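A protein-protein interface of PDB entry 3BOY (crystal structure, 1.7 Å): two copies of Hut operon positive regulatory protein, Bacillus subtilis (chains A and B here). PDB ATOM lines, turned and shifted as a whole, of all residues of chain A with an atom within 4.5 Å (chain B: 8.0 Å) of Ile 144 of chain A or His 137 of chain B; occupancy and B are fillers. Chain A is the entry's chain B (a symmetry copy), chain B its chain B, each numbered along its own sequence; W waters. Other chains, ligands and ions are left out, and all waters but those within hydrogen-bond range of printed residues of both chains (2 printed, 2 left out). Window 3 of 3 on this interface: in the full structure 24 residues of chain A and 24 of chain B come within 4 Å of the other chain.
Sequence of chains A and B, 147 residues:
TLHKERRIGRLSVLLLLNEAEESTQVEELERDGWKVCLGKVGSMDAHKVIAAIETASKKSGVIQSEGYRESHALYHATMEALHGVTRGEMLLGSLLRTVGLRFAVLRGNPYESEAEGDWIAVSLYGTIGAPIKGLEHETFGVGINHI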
ATOM      1  N   GLY A   9      31.845   9.538  12.431  1.00  0.00           N
ATOM      2  CA  GLY A   9      30.474   9.724  11.940  1.00  0.00           C
ATOM      3  C   GLY A   9      30.036  11.172  12.043  1.00  0.00           C
ATOM      4  O   GLY A   9      29.626  11.763  11.067  1.00  0.00           O
ATOM      5  N   GLU A  80      24.894   0.529   4.131  1.00  0.00           N
ATOM      6  CA  GLU A  80      24.338   0.984   5.425  1.00  0.00           C
ATOM      7  C   GLU A  80      23.845   2.442   5.351  1.00  0.00           C
ATOM      8  O   GLU A  80      22.763   2.784   5.833  1.00  0.00           O
ATOM      9  CB  GLU A  80      25.325   0.691   6.573  1.00  0.00           C
ATOM     10  CG  GLU A  80      25.570  -0.834   6.781  1.00  0.00           C
ATOM     11  CD  GLU A  80      26.184  -1.250   8.147  1.00  0.00           C
ATOM     12  OE1 GLU A  80      26.293  -0.369   8.986  1.00  0.00           O
ATOM     13  N   TYR A 111      38.949   5.515  17.387  1.00  0.00           N
ATOM     14  CA  TYR A 111      39.054   4.954  18.745  1.00  0.00           C
ATOM     15  C   TYR A 111      40.282   5.453  19.488  1.00  0.00           C
ATOM     16  O   TYR A 111      41.205   5.958  18.862  1.00  0.00           O
ATOM     17  CB  TYR A 111      39.072   3.419  18.705  1.00  0.00           C
ATOM     18  CG  TYR A 111      37.753   2.898  18.187  1.00  0.00           C
ATOM     19  CD1 TYR A 111      37.550   2.650  16.831  1.00  0.00           C
ATOM     20  CD2 TYR A 111      36.687   2.724  19.050  1.00  0.00           C
ATOM     21  CE1 TYR A 111      36.284   2.200  16.364  1.00  0.00           C
ATOM     22  CE2 TYR A 111      35.443   2.276  18.590  1.00  0.00           C
ATOM     23  CZ  TYR A 111      35.249   2.027  17.241  1.00  0.00           C
ATOM     24  OH  TYR A 111      33.992   1.603  16.796  1.00  0.00           O
ATOM     25  N   TRP A 119      38.818   2.865  10.106  1.00  0.00           N
ATOM     26  CA  TRP A 119      37.375   2.671   9.866  1.00  0.00           C
ATOM     27  C   TRP A 119      36.948   3.667   8.805  1.00  0.00           C
ATOM     28  O   TRP A 119      37.657   4.629   8.509  1.00  0.00           O
ATOM     29  CB  TRP A 119      36.591   2.918  11.157  1.00  0.00           C
ATOM     30  CG  TRP A 119      36.845   1.846  12.179  1.00  0.00           C
ATOM     31  CD1 TRP A 119      38.032   1.548  12.794  1.00  0.00           C
ATOM     32  CD2 TRP A 119      35.894   0.926  12.689  1.00  0.00           C
ATOM     33  NE1 TRP A 119      37.882   0.490  13.630  1.00  0.00           N
ATOM     34  CE2 TRP A 119      36.568   0.089  13.597  1.00  0.00           C
ATOM     35  CE3 TRP A 119      34.518   0.719  12.459  1.00  0.00           C
ATOM     36  CZ2 TRP A 119      35.923  -0.943  14.289  1.00  0.00           C
ATOM     37  CZ3 TRP A 119      33.882  -0.293  13.134  1.00  0.00           C
ATOM     38  CH2 TRP A 119      34.577  -1.124  14.044  1.00  0.00           C
ATOM     39  N   ILE A 120      35.769   3.450   8.224  1.00  0.00           N
ATOM     40  CA  ILE A 120      35.308   4.303   7.152  1.00  0.00           C
ATOM     41  C   ILE A 120      33.851   4.678   7.421  1.00  0.00           C
ATOM     42  O   ILE A 120      33.069   3.831   7.885  1.00  0.00           O
ATOM     43  CB  ILE A 120      35.501   3.606   5.756  1.00  0.00           C
ATOM     44  CG1 ILE A 120      35.254   4.575   4.608  1.00  0.00           C
ATOM     45  CG2 ILE A 120      34.665   2.305   5.663  1.00  0.00           C
ATOM     46  CD1 ILE A 120      36.039   4.244   3.315  1.00  0.00           C
ATOM     47  N   ALA A 121      33.542   5.942   7.168  1.00  0.00           N
ATOM     48  CA  ALA A 121      32.175   6.462   7.267  1.00  0.00           C
ATOM     49  C   ALA A 121      31.765   7.038   5.923  1.00  0.00           C
ATOM     50  O   ALA A 121      32.548   7.764   5.280  1.00  0.00           O
ATOM     51  CB  ALA A 121      32.063   7.507   8.360  1.00  0.00           C
ATOM     52  N   VAL A 142      23.947   7.488   7.174  1.00  0.00           N
ATOM     53  CA  VAL A 142      25.342   7.275   7.550  1.00  0.00           C
ATOM     54  C   VAL A 142      25.618   5.795   7.755  1.00  0.00           C
ATOM     55  O   VAL A 142      24.875   5.115   8.482  1.00  0.00           O
ATOM     56  CB  VAL A 142      25.640   8.014   8.878  1.00  0.00           C
ATOM     57  CG1 VAL A 142      27.103   7.756   9.331  1.00  0.00           C
ATOM     58  CG2 VAL A 142      25.412   9.505   8.663  1.00  0.00           C
ATOM     59  N   GLY A 143      26.690   5.310   7.125  1.00  0.00           N
ATOM     60  CA  GLY A 143      27.127   3.923   7.316  1.00  0.00           C
ATOM     61  C   GLY A 143      28.556   3.939   7.814  1.00  0.00           C
ATOM     62  O   GLY A 143      29.362   4.742   7.341  1.00  0.00           O
ATOM     63  N   ILE A 144      28.866   3.033   8.738  1.00  0.00           N
ATOM     64  CA  ILE A 144      30.222   2.973   9.307  1.00  0.00           C
ATOM     65  C   ILE A 144      30.736   1.546   9.250  1.00  0.00           C
ATOM     66  O   ILE A 144      30.024   0.607   9.587  1.00  0.00           O
ATOM     67  CB  ILE A 144      30.185   3.547  10.756  1.00  0.00           C
ATOM     68  CG1 ILE A 144      30.040   5.102  10.651  1.00  0.00           C
ATOM     69  CG2 ILE A 144      31.459   3.244  11.536  1.00  0.00           C
ATOM     70  CD1 ILE A 144      29.541   5.834  11.873  1.00  0.00           C
ATOM     71  N   ASN A 145      31.973   1.351   8.800  1.00  0.00           N
ATOM     72  CA  ASN A 145      32.532   0.012   8.741  1.00  0.00           C
ATOM     73  C   ASN A 145      34.028  -0.011   9.091  1.00  0.00           C
ATOM     74  O   ASN A 145      34.679   1.017   8.984  1.00  0.00           O
ATOM     75  CB  ASN A 145      32.314  -0.553   7.323  1.00  0.00           C
ATOM     76  CG  ASN A 145      32.285  -2.050   7.283  1.00  0.00           C
ATOM     77  OD1 ASN A 145      32.299  -2.742   8.310  1.00  0.00           O
ATOM     78  ND2 ASN A 145      32.233  -2.587   6.071  1.00  0.00           N
ATOM     79  N   VAL B  85      19.229   4.130  12.003  1.00  0.00           N
ATOM     80  CA  VAL B  85      19.885   3.639  13.186  1.00  0.00           C
ATOM     81  C   VAL B  85      20.113   2.120  13.134  1.00  0.00           C
ATOM     82  O   VAL B  85      21.211   1.677  13.462  1.00  0.00           O
ATOM     83  CB  VAL B  85      19.109   4.050  14.474  1.00  0.00           C
ATOM     84  CG1 VAL B  85      19.716   3.388  15.734  1.00  0.00           C
ATOM     85  CG2 VAL B  85      19.097   5.582  14.610  1.00  0.00           C
ATOM     86  N   ARG B  87      19.435  -0.105  10.342  1.00  0.00           N
ATOM     87  CA  ARG B  87      20.030  -0.572   9.065  1.00  0.00           C
ATOM     88  C   ARG B  87      19.641  -2.018   8.669  1.00  0.00           C
ATOM     89  O   ARG B  87      20.487  -2.838   8.272  1.00  0.00           O
ATOM     90  CB  ARG B  87      21.533  -0.306   9.051  1.00  0.00           C
ATOM     91  CG  ARG B  87      21.883   1.191   8.962  1.00  0.00           C
ATOM     92  CD  ARG B  87      23.176   1.502   9.716  1.00  0.00           C
ATOM     93  NE  ARG B  87      23.039   1.165  11.159  1.00  0.00           N
ATOM     94  CZ  ARG B  87      23.754   0.260  11.812  1.00  0.00           C
ATOM     95  NH1 ARG B  87      24.708  -0.473  11.199  1.00  0.00           N
ATOM     96  NH2 ARG B  87      23.477   0.031  13.092  1.00  0.00           N
ATOM     97  N   ARG B  97      22.352  -6.207  20.584  1.00  0.00           N
ATOM     98  CA  ARG B  97      22.886  -4.858  20.534  1.00  0.00           C
ATOM     99  C   ARG B  97      22.093  -3.827  21.348  1.00  0.00           C
ATOM    100  O   ARG B  97      20.899  -4.002  21.658  1.00  0.00           O
ATOM    101  CB  ARG B  97      23.100  -4.424  19.072  1.00  0.00           C
ATOM    102  CG  ARG B  97      21.852  -4.265  18.259  1.00  0.00           C
ATOM    103  CD  ARG B  97      22.208  -3.805  16.773  1.00  0.00           C
ATOM    104  NE  ARG B  97      20.969  -3.797  16.015  1.00  0.00           N
ATOM    105  CZ  ARG B  97      20.876  -3.539  14.711  1.00  0.00           C
ATOM    106  NH1 ARG B  97      21.968  -3.189  14.007  1.00  0.00           N
ATOM    107  NH2 ARG B  97      19.669  -3.623  14.142  1.00  0.00           N
ATOM    108  N   THR B  98      22.774  -2.744  21.684  1.00  0.00           N
ATOM    109  CA  THR B  98      22.186  -1.702  22.518  1.00  0.00           C
ATOM    110  C   THR B  98      22.478  -0.370  21.838  1.00  0.00           C
ATOM    111  O   THR B  98      23.487  -0.269  21.133  1.00  0.00           O
ATOM    112  CB  THR B  98      22.868  -1.761  23.944  1.00  0.00           C
ATOM    113  OG1 THR B  98      22.444  -0.626  24.725  1.00  0.00           O
ATOM    114  CG2 THR B  98      24.391  -1.750  23.830  1.00  0.00           C
ATOM    115  N   VAL B  99      21.651   0.651  22.101  1.00  0.00           N
ATOM    116  CA  VAL B  99      21.935   2.009  21.637  1.00  0.00           C
ATOM    117  C   VAL B  99      21.890   3.019  22.756  1.00  0.00           C
ATOM    118  O   VAL B  99      21.113   2.844  23.685  1.00  0.00           O
ATOM    119  CB  VAL B  99      20.908   2.542  20.619  1.00  0.00           C
ATOM    120  CG1 VAL B  99      21.016   1.802  19.326  1.00  0.00           C
ATOM    121  CG2 VAL B  99      19.441   2.570  21.182  1.00  0.00           C
ATOM    122  N   GLY B 100      22.694   4.068  22.600  1.00  0.00           N
ATOM    123  CA  GLY B 100      22.628   5.270  23.445  1.00  0.00           C
ATOM    124  C   GLY B 100      22.497   6.427  22.484  1.00  0.00           C
ATOM    125  O   GLY B 100      23.385   6.637  21.652  1.00  0.00           O
ATOM    126  N   TYR B 125      21.140  10.529  17.008  1.00  0.00           N
ATOM    127  CA  TYR B 125      22.592  10.386  16.916  1.00  0.00           C
ATOM    128  C   TYR B 125      23.130   9.767  18.209  1.00  0.00           C
ATOM    129  O   TYR B 125      22.755  10.179  19.320  1.00  0.00           O
ATOM    130  CB  TYR B 125      23.308  11.715  16.619  1.00  0.00           C
ATOM    131  CG  TYR B 125      24.792  11.567  16.816  1.00  0.00           C
ATOM    132  CD1 TYR B 125      25.565  10.842  15.916  1.00  0.00           C
ATOM    133  CD2 TYR B 125      25.426  12.103  17.932  1.00  0.00           C
ATOM    134  CE1 TYR B 125      26.949  10.654  16.102  1.00  0.00           C
ATOM    135  CE2 TYR B 125      26.816  11.937  18.140  1.00  0.00           C
ATOM    136  CZ  TYR B 125      27.570  11.217  17.216  1.00  0.00           C
ATOM    137  OH  TYR B 125      28.918  11.024  17.394  1.00  0.00           O
ATOM    138  N   GLY B 126      23.978   8.756  18.070  1.00  0.00           N
ATOM    139  CA  GLY B 126      24.647   8.192  19.224  1.00  0.00           C
ATOM    140  C   GLY B 126      25.522   7.051  18.821  1.00  0.00           C
ATOM    141  O   GLY B 126      26.183   7.101  17.757  1.00  0.00           O
ATOM    142  N   THR B 127      25.484   6.012  19.634  1.00  0.00           N
ATOM    143  CA  THR B 127      26.262   4.809  19.394  1.00  0.00           C
ATOM    144  C   THR B 127      25.391   3.537  19.498  1.00  0.00           C
ATOM    145  O   THR B 127      24.364   3.514  20.193  1.00  0.00           O
ATOM    146  CB  THR B 127      27.455   4.704  20.417  1.00  0.00           C
ATOM    147  OG1 THR B 127      26.925   4.725  21.769  1.00  0.00           O
ATOM    148  CG2 THR B 127      28.486   5.835  20.190  1.00  0.00           C
ATOM    149  N   ILE B 128      25.764   2.510  18.730  1.00  0.00           N
ATOM    150  CA  ILE B 128      25.099   1.206  18.752  1.00  0.00           C
ATOM    151  C   ILE B 128      26.239   0.210  18.881  1.00  0.00           C
ATOM    152  O   ILE B 128      27.342   0.428  18.322  1.00  0.00           O
ATOM    153  CB  ILE B 128      24.257   1.023  17.442  1.00  0.00           C
ATOM    154  CG1 ILE B 128      23.376  -0.227  17.504  1.00  0.00           C
ATOM    155  CG2 ILE B 128      25.180   1.115  16.241  1.00  0.00           C
ATOM    156  CD1 ILE B 128      22.283  -0.257  16.411  1.00  0.00           C
ATOM    157  N   GLY B 129      26.029  -0.853  19.635  1.00  0.00           N
ATOM    158  CA  GLY B 129      27.133  -1.767  19.859  1.00  0.00           C
ATOM    159  C   GLY B 129      26.730  -3.001  20.584  1.00  0.00           C
ATOM    160  O   GLY B 129      25.548  -3.169  20.909  1.00  0.00           O
ATOM    161  N   ALA B 130      27.707  -3.858  20.845  1.00  0.00           N
ATOM    162  CA  ALA B 130      27.520  -5.005  21.767  1.00  0.00           C
ATOM    163  C   ALA B 130      27.254  -4.399  23.162  1.00  0.00           C
ATOM    164  O   ALA B 130      27.615  -3.252  23.369  1.00  0.00           O
ATOM    165  CB  ALA B 130      28.745  -5.867  21.797  1.00  0.00           C
ATOM    166  N   GLY B 134      32.231   0.390  24.931  1.00  0.00           N
ATOM    167  CA  GLY B 134      33.356   0.575  24.041  1.00  0.00           C
ATOM    168  C   GLY B 134      33.325  -0.256  22.764  1.00  0.00           C
ATOM    169  O   GLY B 134      34.005   0.086  21.775  1.00  0.00           O
ATOM    170  N   LEU B 135      32.589  -1.353  22.819  1.00  0.00           N
ATOM    171  CA  LEU B 135      32.388  -2.238  21.671  1.00  0.00           C
ATOM    172  C   LEU B 135      31.235  -1.663  20.873  1.00  0.00           C
ATOM    173  O   LEU B 135      30.147  -2.236  20.829  1.00  0.00           O
ATOM    174  CB  LEU B 135      32.072  -3.661  22.125  1.00  0.00           C
ATOM    175  CG  LEU B 135      33.192  -4.468  22.812  1.00  0.00           C
ATOM    176  CD1 LEU B 135      32.908  -5.946  22.713  1.00  0.00           C
ATOM    177  CD2 LEU B 135      34.537  -4.159  22.220  1.00  0.00           C
ATOM    178  N   GLU B 136      31.479  -0.509  20.267  1.00  0.00           N
ATOM    179  CA  GLU B 136      30.385   0.273  19.657  1.00  0.00           C
ATOM    180  C   GLU B 136      30.923   1.198  18.587  1.00  0.00           C
ATOM    181  O   GLU B 136      32.112   1.507  18.574  1.00  0.00           O
ATOM    182  CB  GLU B 136      29.687   1.125  20.736  1.00  0.00           C
ATOM    183  CG  GLU B 136      30.629   2.182  21.408  1.00  0.00           C
ATOM    184  CD  GLU B 136      30.201   2.569  22.824  1.00  0.00           C
ATOM    185  OE1 GLU B 136      29.845   1.657  23.594  1.00  0.00           O
ATOM    186  OE2 GLU B 136      30.234   3.783  23.140  1.00  0.00           O
ATOM    187  N   HIS B 137      30.044   1.607  17.677  1.00  0.00           N
ATOM    188  CA  HIS B 137      30.309   2.705  16.759  1.00  0.00           C
ATOM    189  C   HIS B 137      29.127   3.640  16.663  1.00  0.00           C
ATOM    190  O   HIS B 137      28.065   3.362  17.236  1.00  0.00           O
ATOM    191  CB  HIS B 137      30.792   2.203  15.351  1.00  0.00           C
ATOM    192  CG  HIS B 137      29.789   1.353  14.608  1.00  0.00           C
ATOM    193  ND1 HIS B 137      28.566   1.837  14.170  1.00  0.00           N
ATOM    194  CD2 HIS B 137      29.860   0.067  14.184  1.00  0.00           C
ATOM    195  CE1 HIS B 137      27.907   0.869  13.557  1.00  0.00           C
ATOM    196  NE2 HIS B 137      28.667  -0.217  13.548  1.00  0.00           N
ATOM    197  N   GLU B 138      29.315   4.755  15.957  1.00  0.00           N
ATOM    198  CA  GLU B 138      28.287   5.791  15.849  1.00  0.00           C
ATOM    199  C   GLU B 138      27.113   5.318  15.019  1.00  0.00           C
ATOM    200  O   GLU B 138      27.233   4.416  14.175  1.00  0.00           O
ATOM    201  CB  GLU B 138      28.849   7.064  15.227  1.00  0.00           C
ATOM    202  CG  GLU B 138      29.762   7.819  16.167  1.00  0.00           C
ATOM    203  CD  GLU B 138      30.625   8.761  15.403  1.00  0.00           C
ATOM    204  OE1 GLU B 138      31.622   8.294  14.797  1.00  0.00           O
ATOM    205  OE2 GLU B 138      30.252   9.943  15.345  1.00  0.00           O
ATOM    206  N   THR B 139      25.984   5.947  15.259  1.00  0.00           N
ATOM    207  CA  THR B 139      24.776   5.637  14.494  1.00  0.00           C
ATOM    208  C   THR B 139      23.966   6.935  14.321  1.00  0.00           C
ATOM    209  O   THR B 139      24.076   7.840  15.148  1.00  0.00           O
ATOM    210  CB  THR B 139      23.983   4.490  15.151  1.00  0.00           C
ATOM    211  OG1 THR B 139      22.958   4.054  14.261  1.00  0.00           O
ATOM    212  CG2 THR B 139      23.336   4.946  16.455  1.00  0.00           C
ATOM    213  N   PHE B 140      23.185   7.038  13.238  1.00  0.00           N
ATOM    214  CA  PHE B 140      22.417   8.234  12.910  1.00  0.00           C
ATOM    215  C   PHE B 140      21.114   7.816  12.225  1.00  0.00           C
ATOM    216  O   PHE B 140      21.061   6.793  11.512  1.00  0.00           O
ATOM    217  CB  PHE B 140      23.079   9.084  11.799  1.00  0.00           C
ATOM    218  CG  PHE B 140      24.206   9.926  12.221  1.00  0.00           C
ATOM    219  CD1 PHE B 140      25.494   9.383  12.337  1.00  0.00           C
ATOM    220  CD2 PHE B 140      24.027  11.308  12.365  1.00  0.00           C
ATOM    221  CE1 PHE B 140      26.583  10.184  12.665  1.00  0.00           C
ATOM    222  CE2 PHE B 140      25.118  12.123  12.698  1.00  0.00           C
ATOM    223  CZ  PHE B 140      26.381  11.567  12.851  1.00  0.00           C
HETATM  224  O   HOH W   1      23.715   4.815  11.007  1.00  0.00           O
HETATM  225  O   HOH W   2      21.466   7.013   8.849  1.00  0.00           O
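The side-chain carboxylate of Glu 138 of chain B is in hydrogen-bond range of the backbone NH of Gly 9 of chain A (2.7 Å).
The guanidinium group (NH1) of Arg 87 of chain B lies within salt-bridge range of the side-chain carboxylate (OE1) of Glu 80 of chain A (2.7 Å).
O of Glu 136 of chain B is in hydrogen-bond range of OH of Tyr 111 of chain A, at 2.6 Å.
No position is printed for both chains.
Of the 8 pairs that touch across the chains among the printed residues, none has its exchanged pair printed and touching as well.
C of Gly 9 of chain A touches CE1 of Phe 140 of chain B (3.6 Å).
His 137 of chain B touches Tyr 111 of chain A (CB to OH, 3.6 Å).
CG2 of Val 142 of chain A touches CD1 of Phe 140 of chain B, 3.7 Å away.
Ile 144 of chain A touches His 137 of chain B.
Glu 138 of chain B touches Ile 144 of chain A.
The side-chain carboxylate (OE1) of Glu 136 of chain B sits at hydrogen-bond distance from the backbone NH (N) of Gly 134 of chain B (3.0 Å).
The backbone NH (N) of Ile 128 of chain B sits at hydrogen-bond distance from the backbone carbonyl oxygen (O) of His 137 of chain B (2.9 Å).
The guanidinium group of Arg 87 of chain B sits at hydrogen-bond distance from the backbone carbonyl oxygen of Val 85 of chain B, at 2.8 Å.
The side-chain carboxylate (OE2) of Glu 138 of chain B lies within hydrogen-bond range of the side-chain hydroxyl (OH) of Tyr 125 of chain B (2.7 Å).
N of Val 85 of chain B lies within hydrogen-bond range of O of Phe 140 of chain B, 3.3 Å away.
Printed residues of chain B within 4 Å of Gly 9 of chain A: Glu 138 (2.7 Å) and Phe 140 (3.6 Å).
Printed residues of chain B within 4 Å of Tyr 111 of chain A: Glu 136 and His 137.
Asn 145 of chain A touches none of the printed residues of chain B.
His 137 of chain B touches two residues of chain A.
The nearest residue of chain A that does not touch His 137 of chain B is Trp 119 of chain A (4.2 Å).
Of the 10 printed residues of chain A, 5 touch a printed residue of chain B.
Hydrophobic or aromatic side chains of chain A within 4 Å of the printed part of chain B: Tyr 111, Val 142 and Ile 144.
Hydrophobic or aromatic side chains of chain B within 4 Å of the printed part of chain A: His 137 and Phe 140.
Water W2 bridges the backbone carbonyl oxygen (O) of Phe 140 of chain B and the backbone NH (N) of Val 142 of chain A.
Water W1 lies within hydrogen-bond range of the backbone carbonyl oxygen (O) of Val 142 of chain A, the backbone NH (N) of Phe 140 of chain B and the side-chain hydroxyl (OG1) of Thr 139 of chain B.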
